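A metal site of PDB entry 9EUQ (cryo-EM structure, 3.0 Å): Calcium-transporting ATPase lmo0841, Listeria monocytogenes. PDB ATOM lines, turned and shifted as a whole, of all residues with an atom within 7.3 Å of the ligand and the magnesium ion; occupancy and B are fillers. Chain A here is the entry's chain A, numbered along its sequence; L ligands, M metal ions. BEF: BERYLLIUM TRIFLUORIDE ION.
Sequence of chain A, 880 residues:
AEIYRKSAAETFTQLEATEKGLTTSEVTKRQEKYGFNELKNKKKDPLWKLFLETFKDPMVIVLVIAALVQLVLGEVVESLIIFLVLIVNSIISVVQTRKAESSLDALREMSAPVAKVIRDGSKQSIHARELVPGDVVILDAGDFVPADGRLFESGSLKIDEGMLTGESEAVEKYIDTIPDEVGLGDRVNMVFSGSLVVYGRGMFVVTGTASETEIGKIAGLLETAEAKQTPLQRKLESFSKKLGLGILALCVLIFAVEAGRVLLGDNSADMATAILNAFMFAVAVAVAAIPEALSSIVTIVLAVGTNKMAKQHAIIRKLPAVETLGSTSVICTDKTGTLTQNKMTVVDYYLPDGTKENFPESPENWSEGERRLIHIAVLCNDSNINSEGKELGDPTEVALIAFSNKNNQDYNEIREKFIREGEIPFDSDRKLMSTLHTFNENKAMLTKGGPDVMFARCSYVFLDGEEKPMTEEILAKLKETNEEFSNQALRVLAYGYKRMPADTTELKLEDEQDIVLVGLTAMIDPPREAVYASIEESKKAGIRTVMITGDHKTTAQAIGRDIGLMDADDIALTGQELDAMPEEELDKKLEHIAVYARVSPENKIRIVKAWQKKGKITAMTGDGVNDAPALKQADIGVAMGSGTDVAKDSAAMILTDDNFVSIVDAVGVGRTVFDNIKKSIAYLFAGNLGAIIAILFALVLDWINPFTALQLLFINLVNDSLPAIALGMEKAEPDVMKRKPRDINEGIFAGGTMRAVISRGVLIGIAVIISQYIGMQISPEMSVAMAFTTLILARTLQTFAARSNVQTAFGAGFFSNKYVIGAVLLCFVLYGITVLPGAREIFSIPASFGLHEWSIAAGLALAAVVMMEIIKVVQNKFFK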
ATOM      1  N   GLY A 162      11.502 -22.505 -23.739  1.00  0.00           N
ATOM      2  CA  GLY A 162      11.098 -21.599 -22.690  1.00  0.00           C
ATOM      3  C   GLY A 162      10.521 -20.281 -23.141  1.00  0.00           C
ATOM      4  O   GLY A 162      10.143 -19.459 -22.307  1.00  0.00           O
ATOM      5  N   LEU A 164       8.022 -20.224 -25.662  1.00  0.00           N
ATOM      6  CA  LEU A 164       6.613 -20.486 -25.928  1.00  0.00           C
ATOM      7  C   LEU A 164       5.942 -21.216 -24.776  1.00  0.00           C
ATOM      8  O   LEU A 164       4.902 -20.779 -24.286  1.00  0.00           O
ATOM      9  CB  LEU A 164       6.454 -21.294 -27.222  1.00  0.00           C
ATOM     10  CG  LEU A 164       7.424 -20.941 -28.340  1.00  0.00           C
ATOM     11  CD1 LEU A 164       7.550 -22.089 -29.307  1.00  0.00           C
ATOM     12  CD2 LEU A 164       6.904 -19.704 -29.059  1.00  0.00           C
ATOM     13  N   THR A 165       6.512 -22.339 -24.335  1.00  0.00           N
ATOM     14  CA  THR A 165       5.992 -23.017 -23.154  1.00  0.00           C
ATOM     15  C   THR A 165       6.281 -22.235 -21.883  1.00  0.00           C
ATOM     16  O   THR A 165       5.569 -22.402 -20.889  1.00  0.00           O
ATOM     17  CB  THR A 165       6.581 -24.425 -23.080  1.00  0.00           C
ATOM     18  OG1 THR A 165       6.431 -25.075 -24.357  1.00  0.00           O
ATOM     19  CG2 THR A 165       5.861 -25.264 -22.034  1.00  0.00           C
ATOM     20  N   GLY A 166       7.290 -21.371 -21.905  1.00  0.00           N
ATOM     21  CA  GLY A 166       7.632 -20.565 -20.743  1.00  0.00           C
ATOM     22  C   GLY A 166       8.437 -21.278 -19.687  1.00  0.00           C
ATOM     23  O   GLY A 166       8.574 -20.739 -18.582  1.00  0.00           O
ATOM     24  N   GLU A 167       8.900 -22.498 -20.000  1.00  0.00           N
ATOM     25  CA  GLU A 167       9.634 -23.340 -19.003  1.00  0.00           C
ATOM     26  C   GLU A 167      11.010 -23.762 -19.502  1.00  0.00           C
ATOM     27  O   GLU A 167      11.091 -24.246 -20.642  1.00  0.00           O
ATOM     28  CB  GLU A 167       8.832 -24.619 -18.767  1.00  0.00           C
ATOM     29  CG  GLU A 167       7.379 -24.502 -19.166  1.00  0.00           C
ATOM     30  CD  GLU A 167       6.389 -25.172 -18.234  1.00  0.00           C
ATOM     31  OE1 GLU A 167       6.758 -26.190 -17.611  1.00  0.00           O
ATOM     32  OE2 GLU A 167       5.249 -24.683 -18.151  1.00  0.00           O
ATOM     33  N   SER A 168      12.051 -23.632 -18.661  1.00  0.00           N
ATOM     34  CA  SER A 168      13.382 -24.074 -19.049  1.00  0.00           C
ATOM     35  C   SER A 168      13.497 -25.593 -18.927  1.00  0.00           C
ATOM     36  O   SER A 168      14.413 -26.108 -18.278  1.00  0.00           O
ATOM     37  CB  SER A 168      14.445 -23.394 -18.179  1.00  0.00           C
ATOM     38  OG  SER A 168      14.775 -24.181 -17.050  1.00  0.00           O
ATOM     39  N   THR A 333      -2.308 -14.239 -15.189  1.00  0.00           N
ATOM     40  CA  THR A 333      -1.071 -14.717 -14.595  1.00  0.00           C
ATOM     41  C   THR A 333      -0.476 -15.861 -15.405  1.00  0.00           C
ATOM     42  O   THR A 333      -1.189 -16.689 -15.972  1.00  0.00           O
ATOM     43  CB  THR A 333      -1.299 -15.191 -13.156  1.00  0.00           C
ATOM     44  OG1 THR A 333      -2.260 -14.335 -12.527  1.00  0.00           O
ATOM     45  CG2 THR A 333      -0.008 -15.143 -12.392  1.00  0.00           C
ATOM     46  N   ASP A 334       0.854 -15.888 -15.452  1.00  0.00           N
ATOM     47  CA  ASP A 334       1.606 -17.041 -15.914  1.00  0.00           C
ATOM     48  C   ASP A 334       1.903 -17.944 -14.722  1.00  0.00           C
ATOM     49  O   ASP A 334       1.953 -17.496 -13.575  1.00  0.00           O
ATOM     50  CB  ASP A 334       2.916 -16.603 -16.586  1.00  0.00           C
ATOM     51  CG  ASP A 334       3.691 -17.757 -17.166  1.00  0.00           C
ATOM     52  OD1 ASP A 334       3.071 -18.730 -17.661  1.00  0.00           O
ATOM     53  OD2 ASP A 334       4.942 -17.701 -17.138  1.00  0.00           O
ATOM     54  N   LYS A 335       2.069 -19.242 -14.997  1.00  0.00           N
ATOM     55  CA  LYS A 335       2.346 -20.194 -13.930  1.00  0.00           C
ATOM     56  C   LYS A 335       3.835 -20.436 -13.751  1.00  0.00           C
ATOM     57  O   LYS A 335       4.384 -20.183 -12.675  1.00  0.00           O
ATOM     58  CB  LYS A 335       1.621 -21.509 -14.202  1.00  0.00           C
ATOM     59  CG  LYS A 335       1.599 -22.466 -13.037  1.00  0.00           C
ATOM     60  CD  LYS A 335       1.433 -23.892 -13.507  1.00  0.00           C
ATOM     61  CE  LYS A 335       2.658 -24.353 -14.255  1.00  0.00           C
ATOM     62  NZ  LYS A 335       3.519 -25.231 -13.414  1.00  0.00           N
ATOM     63  N   THR A 336       4.506 -20.911 -14.787  1.00  0.00           N
ATOM     64  CA  THR A 336       5.919 -21.263 -14.692  1.00  0.00           C
ATOM     65  C   THR A 336       6.752 -19.981 -14.670  1.00  0.00           C
ATOM     66  O   THR A 336       6.878 -19.300 -15.696  1.00  0.00           O
ATOM     67  CB  THR A 336       6.327 -22.158 -15.855  1.00  0.00           C
ATOM     68  OG1 THR A 336       5.416 -23.265 -15.937  1.00  0.00           O
ATOM     69  CG2 THR A 336       7.732 -22.692 -15.647  1.00  0.00           C
ATOM     70  N   GLY A 337       7.326 -19.674 -13.509  1.00  0.00           N
ATOM     71  CA  GLY A 337       8.158 -18.508 -13.350  1.00  0.00           C
ATOM     72  C   GLY A 337       7.467 -17.308 -12.731  1.00  0.00           C
ATOM     73  O   GLY A 337       8.142 -16.399 -12.240  1.00  0.00           O
ATOM     74  N   THR A 338       6.137 -17.284 -12.739  1.00  0.00           N
ATOM     75  CA  THR A 338       5.370 -16.183 -12.168  1.00  0.00           C
ATOM     76  C   THR A 338       4.582 -16.622 -10.935  1.00  0.00           C
ATOM     77  O   THR A 338       4.748 -16.043  -9.857  1.00  0.00           O
ATOM     78  CB  THR A 338       4.429 -15.588 -13.214  1.00  0.00           C
ATOM     79  OG1 THR A 338       5.145 -15.392 -14.433  1.00  0.00           O
ATOM     80  CG2 THR A 338       3.868 -14.256 -12.739  1.00  0.00           C
ATOM     81  N   LEU A 339       3.740 -17.644 -11.071  1.00  0.00           N
ATOM     82  CA  LEU A 339       3.114 -18.248  -9.892  1.00  0.00           C
ATOM     83  C   LEU A 339       4.089 -19.184  -9.202  1.00  0.00           C
ATOM     84  O   LEU A 339       4.382 -19.028  -8.010  1.00  0.00           O
ATOM     85  CB  LEU A 339       1.843 -19.000 -10.295  1.00  0.00           C
ATOM     86  CG  LEU A 339       0.597 -18.150 -10.511  1.00  0.00           C
ATOM     87  CD1 LEU A 339      -0.630 -19.036 -10.538  1.00  0.00           C
ATOM     88  CD2 LEU A 339       0.465 -17.102  -9.422  1.00  0.00           C
ATOM     89  N   THR A 340       4.603 -20.172  -9.941  1.00  0.00           N
ATOM     90  CA  THR A 340       5.664 -21.016  -9.420  1.00  0.00           C
ATOM     91  C   THR A 340       7.005 -20.294  -9.555  1.00  0.00           C
ATOM     92  O   THR A 340       7.108 -19.213 -10.138  1.00  0.00           O
ATOM     93  CB  THR A 340       5.676 -22.360 -10.151  1.00  0.00           C
ATOM     94  OG1 THR A 340       6.497 -22.256 -11.320  1.00  0.00           O
ATOM     95  CG2 THR A 340       4.271 -22.757 -10.566  1.00  0.00           C
ATOM     96  N   ASN A 342       9.615 -21.438 -11.181  1.00  0.00           N
ATOM     97  CA  ASN A 342      10.316 -22.000 -12.326  1.00  0.00           C
ATOM     98  C   ASN A 342      11.444 -22.940 -11.897  1.00  0.00           C
ATOM     99  O   ASN A 342      12.354 -23.217 -12.678  1.00  0.00           O
ATOM    100  CB  ASN A 342      10.862 -20.906 -13.252  1.00  0.00           C
ATOM    101  CG  ASN A 342      10.938 -21.358 -14.701  1.00  0.00           C
ATOM    102  OD1 ASN A 342      10.952 -22.552 -14.998  1.00  0.00           O
ATOM    103  ND2 ASN A 342      10.987 -20.387 -15.614  1.00  0.00           N
ATOM    104  N   MET A 547      -5.212 -17.673 -14.750  1.00  0.00           N
ATOM    105  CA  MET A 547      -3.920 -18.278 -15.029  1.00  0.00           C
ATOM    106  C   MET A 547      -3.825 -18.624 -16.502  1.00  0.00           C
ATOM    107  O   MET A 547      -4.648 -19.388 -17.021  1.00  0.00           O
ATOM    108  CB  MET A 547      -3.704 -19.525 -14.171  1.00  0.00           C
ATOM    109  CG  MET A 547      -2.316 -19.588 -13.569  1.00  0.00           C
ATOM    110  SD  MET A 547      -1.731 -21.257 -13.241  1.00  0.00           S
ATOM    111  CE  MET A 547      -3.205 -22.030 -12.611  1.00  0.00           C
ATOM    112  N   ILE A 548      -2.823 -18.074 -17.170  1.00  0.00           N
ATOM    113  CA  ILE A 548      -2.524 -18.380 -18.566  1.00  0.00           C
ATOM    114  C   ILE A 548      -1.092 -18.902 -18.600  1.00  0.00           C
ATOM    115  O   ILE A 548      -0.142 -18.156 -18.347  1.00  0.00           O
ATOM    116  CB  ILE A 548      -2.676 -17.150 -19.474  1.00  0.00           C
ATOM    117  CG1 ILE A 548      -3.834 -16.276 -18.996  1.00  0.00           C
ATOM    118  CG2 ILE A 548      -2.906 -17.569 -20.896  1.00  0.00           C
ATOM    119  CD1 ILE A 548      -3.892 -14.935 -19.670  1.00  0.00           C
ATOM    120  N   THR A 549      -0.936 -20.182 -18.933  1.00  0.00           N
ATOM    121  CA  THR A 549       0.366 -20.832 -18.833  1.00  0.00           C
ATOM    122  C   THR A 549       0.580 -21.792 -19.997  1.00  0.00           C
ATOM    123  O   THR A 549      -0.378 -22.282 -20.603  1.00  0.00           O
ATOM    124  CB  THR A 549       0.515 -21.578 -17.515  1.00  0.00           C
ATOM    125  OG1 THR A 549       1.790 -22.241 -17.484  1.00  0.00           O
ATOM    126  CG2 THR A 549      -0.591 -22.610 -17.363  1.00  0.00           C
ATOM    127  N   GLY A 550       1.847 -22.051 -20.293  1.00  0.00           N
ATOM    128  CA  GLY A 550       2.252 -22.999 -21.294  1.00  0.00           C
ATOM    129  C   GLY A 550       2.341 -24.436 -20.829  1.00  0.00           C
ATOM    130  O   GLY A 550       2.614 -25.322 -21.654  1.00  0.00           O
ATOM    131  N   ASP A 551       2.128 -24.705 -19.548  1.00  0.00           N
ATOM    132  CA  ASP A 551       2.192 -26.062 -19.041  1.00  0.00           C
ATOM    133  C   ASP A 551       0.967 -26.865 -19.496  1.00  0.00           C
ATOM    134  O   ASP A 551      -0.003 -26.329 -20.029  1.00  0.00           O
ATOM    135  CB  ASP A 551       2.275 -26.087 -17.509  1.00  0.00           C
ATOM    136  CG  ASP A 551       3.409 -26.958 -17.000  1.00  0.00           C
ATOM    137  OD1 ASP A 551       3.796 -27.904 -17.721  1.00  0.00           O
ATOM    138  OD2 ASP A 551       3.936 -26.693 -15.897  1.00  0.00           O
ATOM    139  N   VAL A 599      -1.067 -22.932 -23.651  1.00  0.00           N
ATOM    140  CA  VAL A 599      -1.394 -21.817 -24.526  1.00  0.00           C
ATOM    141  C   VAL A 599      -0.127 -21.277 -25.180  1.00  0.00           C
ATOM    142  O   VAL A 599       0.975 -21.365 -24.626  1.00  0.00           O
ATOM    143  CB  VAL A 599      -2.127 -20.700 -23.757  1.00  0.00           C
ATOM    144  CG1 VAL A 599      -3.340 -21.262 -23.027  1.00  0.00           C
ATOM    145  CG2 VAL A 599      -1.194 -20.030 -22.771  1.00  0.00           C
ATOM    146  N   LYS A 604      -2.246 -16.109 -25.185  1.00  0.00           N
ATOM    147  CA  LYS A 604      -2.216 -15.196 -24.042  1.00  0.00           C
ATOM    148  C   LYS A 604      -2.702 -13.806 -24.446  1.00  0.00           C
ATOM    149  O   LYS A 604      -3.494 -13.184 -23.716  1.00  0.00           O
ATOM    150  CB  LYS A 604      -0.806 -15.116 -23.460  1.00  0.00           C
ATOM    151  CG  LYS A 604      -0.242 -16.452 -23.015  1.00  0.00           C
ATOM    152  CD  LYS A 604       0.579 -16.307 -21.758  1.00  0.00           C
ATOM    153  CE  LYS A 604       1.316 -17.585 -21.422  1.00  0.00           C
ATOM    154  NZ  LYS A 604       1.788 -17.591 -20.016  1.00  0.00           N
ATOM    155  N   MET A 620      -2.065  -8.579 -16.661  1.00  0.00           N
ATOM    156  CA  MET A 620      -1.277  -9.739 -17.052  1.00  0.00           C
ATOM    157  C   MET A 620       0.067  -9.691 -16.331  1.00  0.00           C
ATOM    158  O   MET A 620       0.789  -8.686 -16.425  1.00  0.00           O
ATOM    159  CB  MET A 620      -1.076  -9.792 -18.553  1.00  0.00           C
ATOM    160  CG  MET A 620      -0.099 -10.859 -18.995  1.00  0.00           C
ATOM    161  SD  MET A 620      -0.840 -12.498 -19.026  1.00  0.00           S
ATOM    162  CE  MET A 620       0.605 -13.508 -19.324  1.00  0.00           C
ATOM    163  N   GLY A 622       3.594 -11.963 -15.862  1.00  0.00           N
ATOM    164  CA  GLY A 622       4.340 -13.079 -16.395  1.00  0.00           C
ATOM    165  C   GLY A 622       5.826 -12.843 -16.290  1.00  0.00           C
ATOM    166  O   GLY A 622       6.290 -11.768 -15.914  1.00  0.00           O
ATOM    167  N   ASP A 623       6.583 -13.891 -16.637  1.00  0.00           N
ATOM    168  CA  ASP A 623       8.035 -13.828 -16.608  1.00  0.00           C
ATOM    169  C   ASP A 623       8.703 -14.348 -17.875  1.00  0.00           C
ATOM    170  O   ASP A 623       9.859 -13.983 -18.123  1.00  0.00           O
ATOM    171  CB  ASP A 623       8.584 -14.621 -15.418  1.00  0.00           C
ATOM    172  CG  ASP A 623       8.764 -16.092 -15.728  1.00  0.00           C
ATOM    173  OD1 ASP A 623       7.837 -16.702 -16.295  1.00  0.00           O
ATOM    174  OD2 ASP A 623       9.847 -16.639 -15.404  1.00  0.00           O
ATOM    175  N   GLY A 624       8.026 -15.163 -18.673  1.00  0.00           N
ATOM    176  CA  GLY A 624       8.624 -15.727 -19.871  1.00  0.00           C
ATOM    177  C   GLY A 624       8.395 -14.859 -21.089  1.00  0.00           C
ATOM    178  O   GLY A 624       7.786 -13.793 -21.037  1.00  0.00           O
ATOM    179  N   VAL A 625       8.901 -15.353 -22.227  1.00  0.00           N
ATOM    180  CA  VAL A 625       8.740 -14.628 -23.479  1.00  0.00           C
ATOM    181  C   VAL A 625       7.273 -14.632 -23.902  1.00  0.00           C
ATOM    182  O   VAL A 625       6.752 -13.629 -24.401  1.00  0.00           O
ATOM    183  CB  VAL A 625       9.631 -15.250 -24.563  1.00  0.00           C
ATOM    184  CG1 VAL A 625       9.045 -15.046 -25.957  1.00  0.00           C
ATOM    185  CG2 VAL A 625      11.040 -14.719 -24.483  1.00  0.00           C
ATOM    186  N   ASN A 626       6.577 -15.753 -23.693  1.00  0.00           N
ATOM    187  CA  ASN A 626       5.190 -15.868 -24.117  1.00  0.00           C
ATOM    188  C   ASN A 626       4.295 -14.847 -23.437  1.00  0.00           C
ATOM    189  O   ASN A 626       3.279 -14.434 -24.006  1.00  0.00           O
ATOM    190  CB  ASN A 626       4.674 -17.281 -23.829  1.00  0.00           C
ATOM    191  CG  ASN A 626       5.097 -17.799 -22.469  1.00  0.00           C
ATOM    192  OD1 ASN A 626       6.105 -17.346 -21.910  1.00  0.00           O
ATOM    193  ND2 ASN A 626       4.345 -18.749 -21.936  1.00  0.00           N
ATOM    194  N   ASP A 627       4.658 -14.410 -22.234  1.00  0.00           N
ATOM    195  CA  ASP A 627       3.880 -13.401 -21.538  1.00  0.00           C
ATOM    196  C   ASP A 627       4.111 -11.999 -22.095  1.00  0.00           C
ATOM    197  O   ASP A 627       3.239 -11.132 -21.923  1.00  0.00           O
ATOM    198  CB  ASP A 627       4.214 -13.411 -20.046  1.00  0.00           C
ATOM    199  CG  ASP A 627       4.229 -14.811 -19.469  1.00  0.00           C
ATOM    200  OD1 ASP A 627       3.215 -15.516 -19.611  1.00  0.00           O
ATOM    201  OD2 ASP A 627       5.262 -15.199 -18.880  1.00  0.00           O
ATOM    202  N   GLY A 643      12.521 -13.222 -14.423  1.00  0.00           N
ATOM    203  CA  GLY A 643      11.993 -13.422 -15.758  1.00  0.00           C
ATOM    204  C   GLY A 643      12.940 -12.932 -16.824  1.00  0.00           C
ATOM    205  O   GLY A 643      13.937 -12.258 -16.566  1.00  0.00           O
HETATM  206 BE   BEF L   1       4.335 -19.932 -18.234  1.00  0.00          BE
HETATM  207  F1  BEF L   1       5.803 -19.934 -18.358  1.00  0.00           F
HETATM  208  F2  BEF L   1       3.705 -20.659 -17.124  1.00  0.00           F
HETATM  209  F3  BEF L   1       3.513 -19.528 -19.397  1.00  0.00           F
HETATM  210 MG    MG M   1       6.899 -18.129 -17.442  1.00  0.00          MG
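OG1 of Thr 549 is in hydrogen-bond range of F2 of the ligand, 2.5 Å away. NZ of Lys 604 sits at hydrogen-bond distance from F3 of the ligand (2.7 Å). OG1 of Thr 336 lies close to F2 of the ligand (3.3 Å). The side-chain carboxylate (OD1) of Asp 334 is bound to a beryllium atom (BE) of the ligand (1.8 Å). The backbone NH (N) of Gly 550 sits at hydrogen-bond distance from a fluorine (F3) of the ligand, at 3.2 Å. A fluorine (F2) of the ligand sits at hydrogen-bond distance from the backbone NH (N) of Thr 336, at 2.5 Å. A fluorine (F3) of the ligand lies within hydrogen-bond range of the side-chain amide nitrogen (ND2) of Asn 626 (2.8 Å). The backbone NH of Lys 335 sits at hydrogen-bond distance from a fluorine (F2) of the ligand (3.0 Å).
The backbone NH (N) of Thr 340 sits at hydrogen-bond distance from the backbone carbonyl oxygen (O) of Lys 335, at 2.7 Å. The side-chain amino group (NZ) of Lys 604 lies close to the side-chain carboxylate (OD1) of Asp 334. The side-chain amino group (NZ) of Lys 604 sits close to the side-chain amide nitrogen (ND2) of Asn 626, at 3.4 Å. The backbone NH (N) of Asp 623 lies within hydrogen-bond range of the side-chain hydroxyl (OG1) of Thr 338, at 3.0 Å. The backbone carbonyl oxygen (O) of Leu 164 sits at hydrogen-bond distance from the side-chain amide nitrogen (ND2) of Asn 626 (3.2 Å). The side-chain carboxylate (OD1) of Asp 627 is in salt-bridge range of the side-chain amino group (NZ) of Lys 604 (2.6 Å). The side-chain carboxylate of Asp 627 is in hydrogen-bond range of the backbone NH of Asp 623 (2.9 Å). O of Asp 334 is in hydrogen-bond range of N of Leu 339 (3.1 Å).
F1 of the ligand sits close to O of Gly 166, at 2.9 Å. Thr 165 touches the ligand. Of the 30 residues printed, 9 come within 4 Å of the ligand. The nearest printed residue that does not touch the ligand is Asp 627 (4.03 Å).
Gly 166 touches the magnesium ion. Gly 624 touches the magnesium ion (N to MG, 3.4 Å). Asp 627 touches the magnesium ion (OD2 to MG, 3.7 Å). The nearest printed residue that does not touch the magnesium ion is Gly 337 (4.2 Å).
The magnesium ion is bound by OD2 of Asp 334, OD1 of Asp 623, O of Thr 336 and F1 of the ligand.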
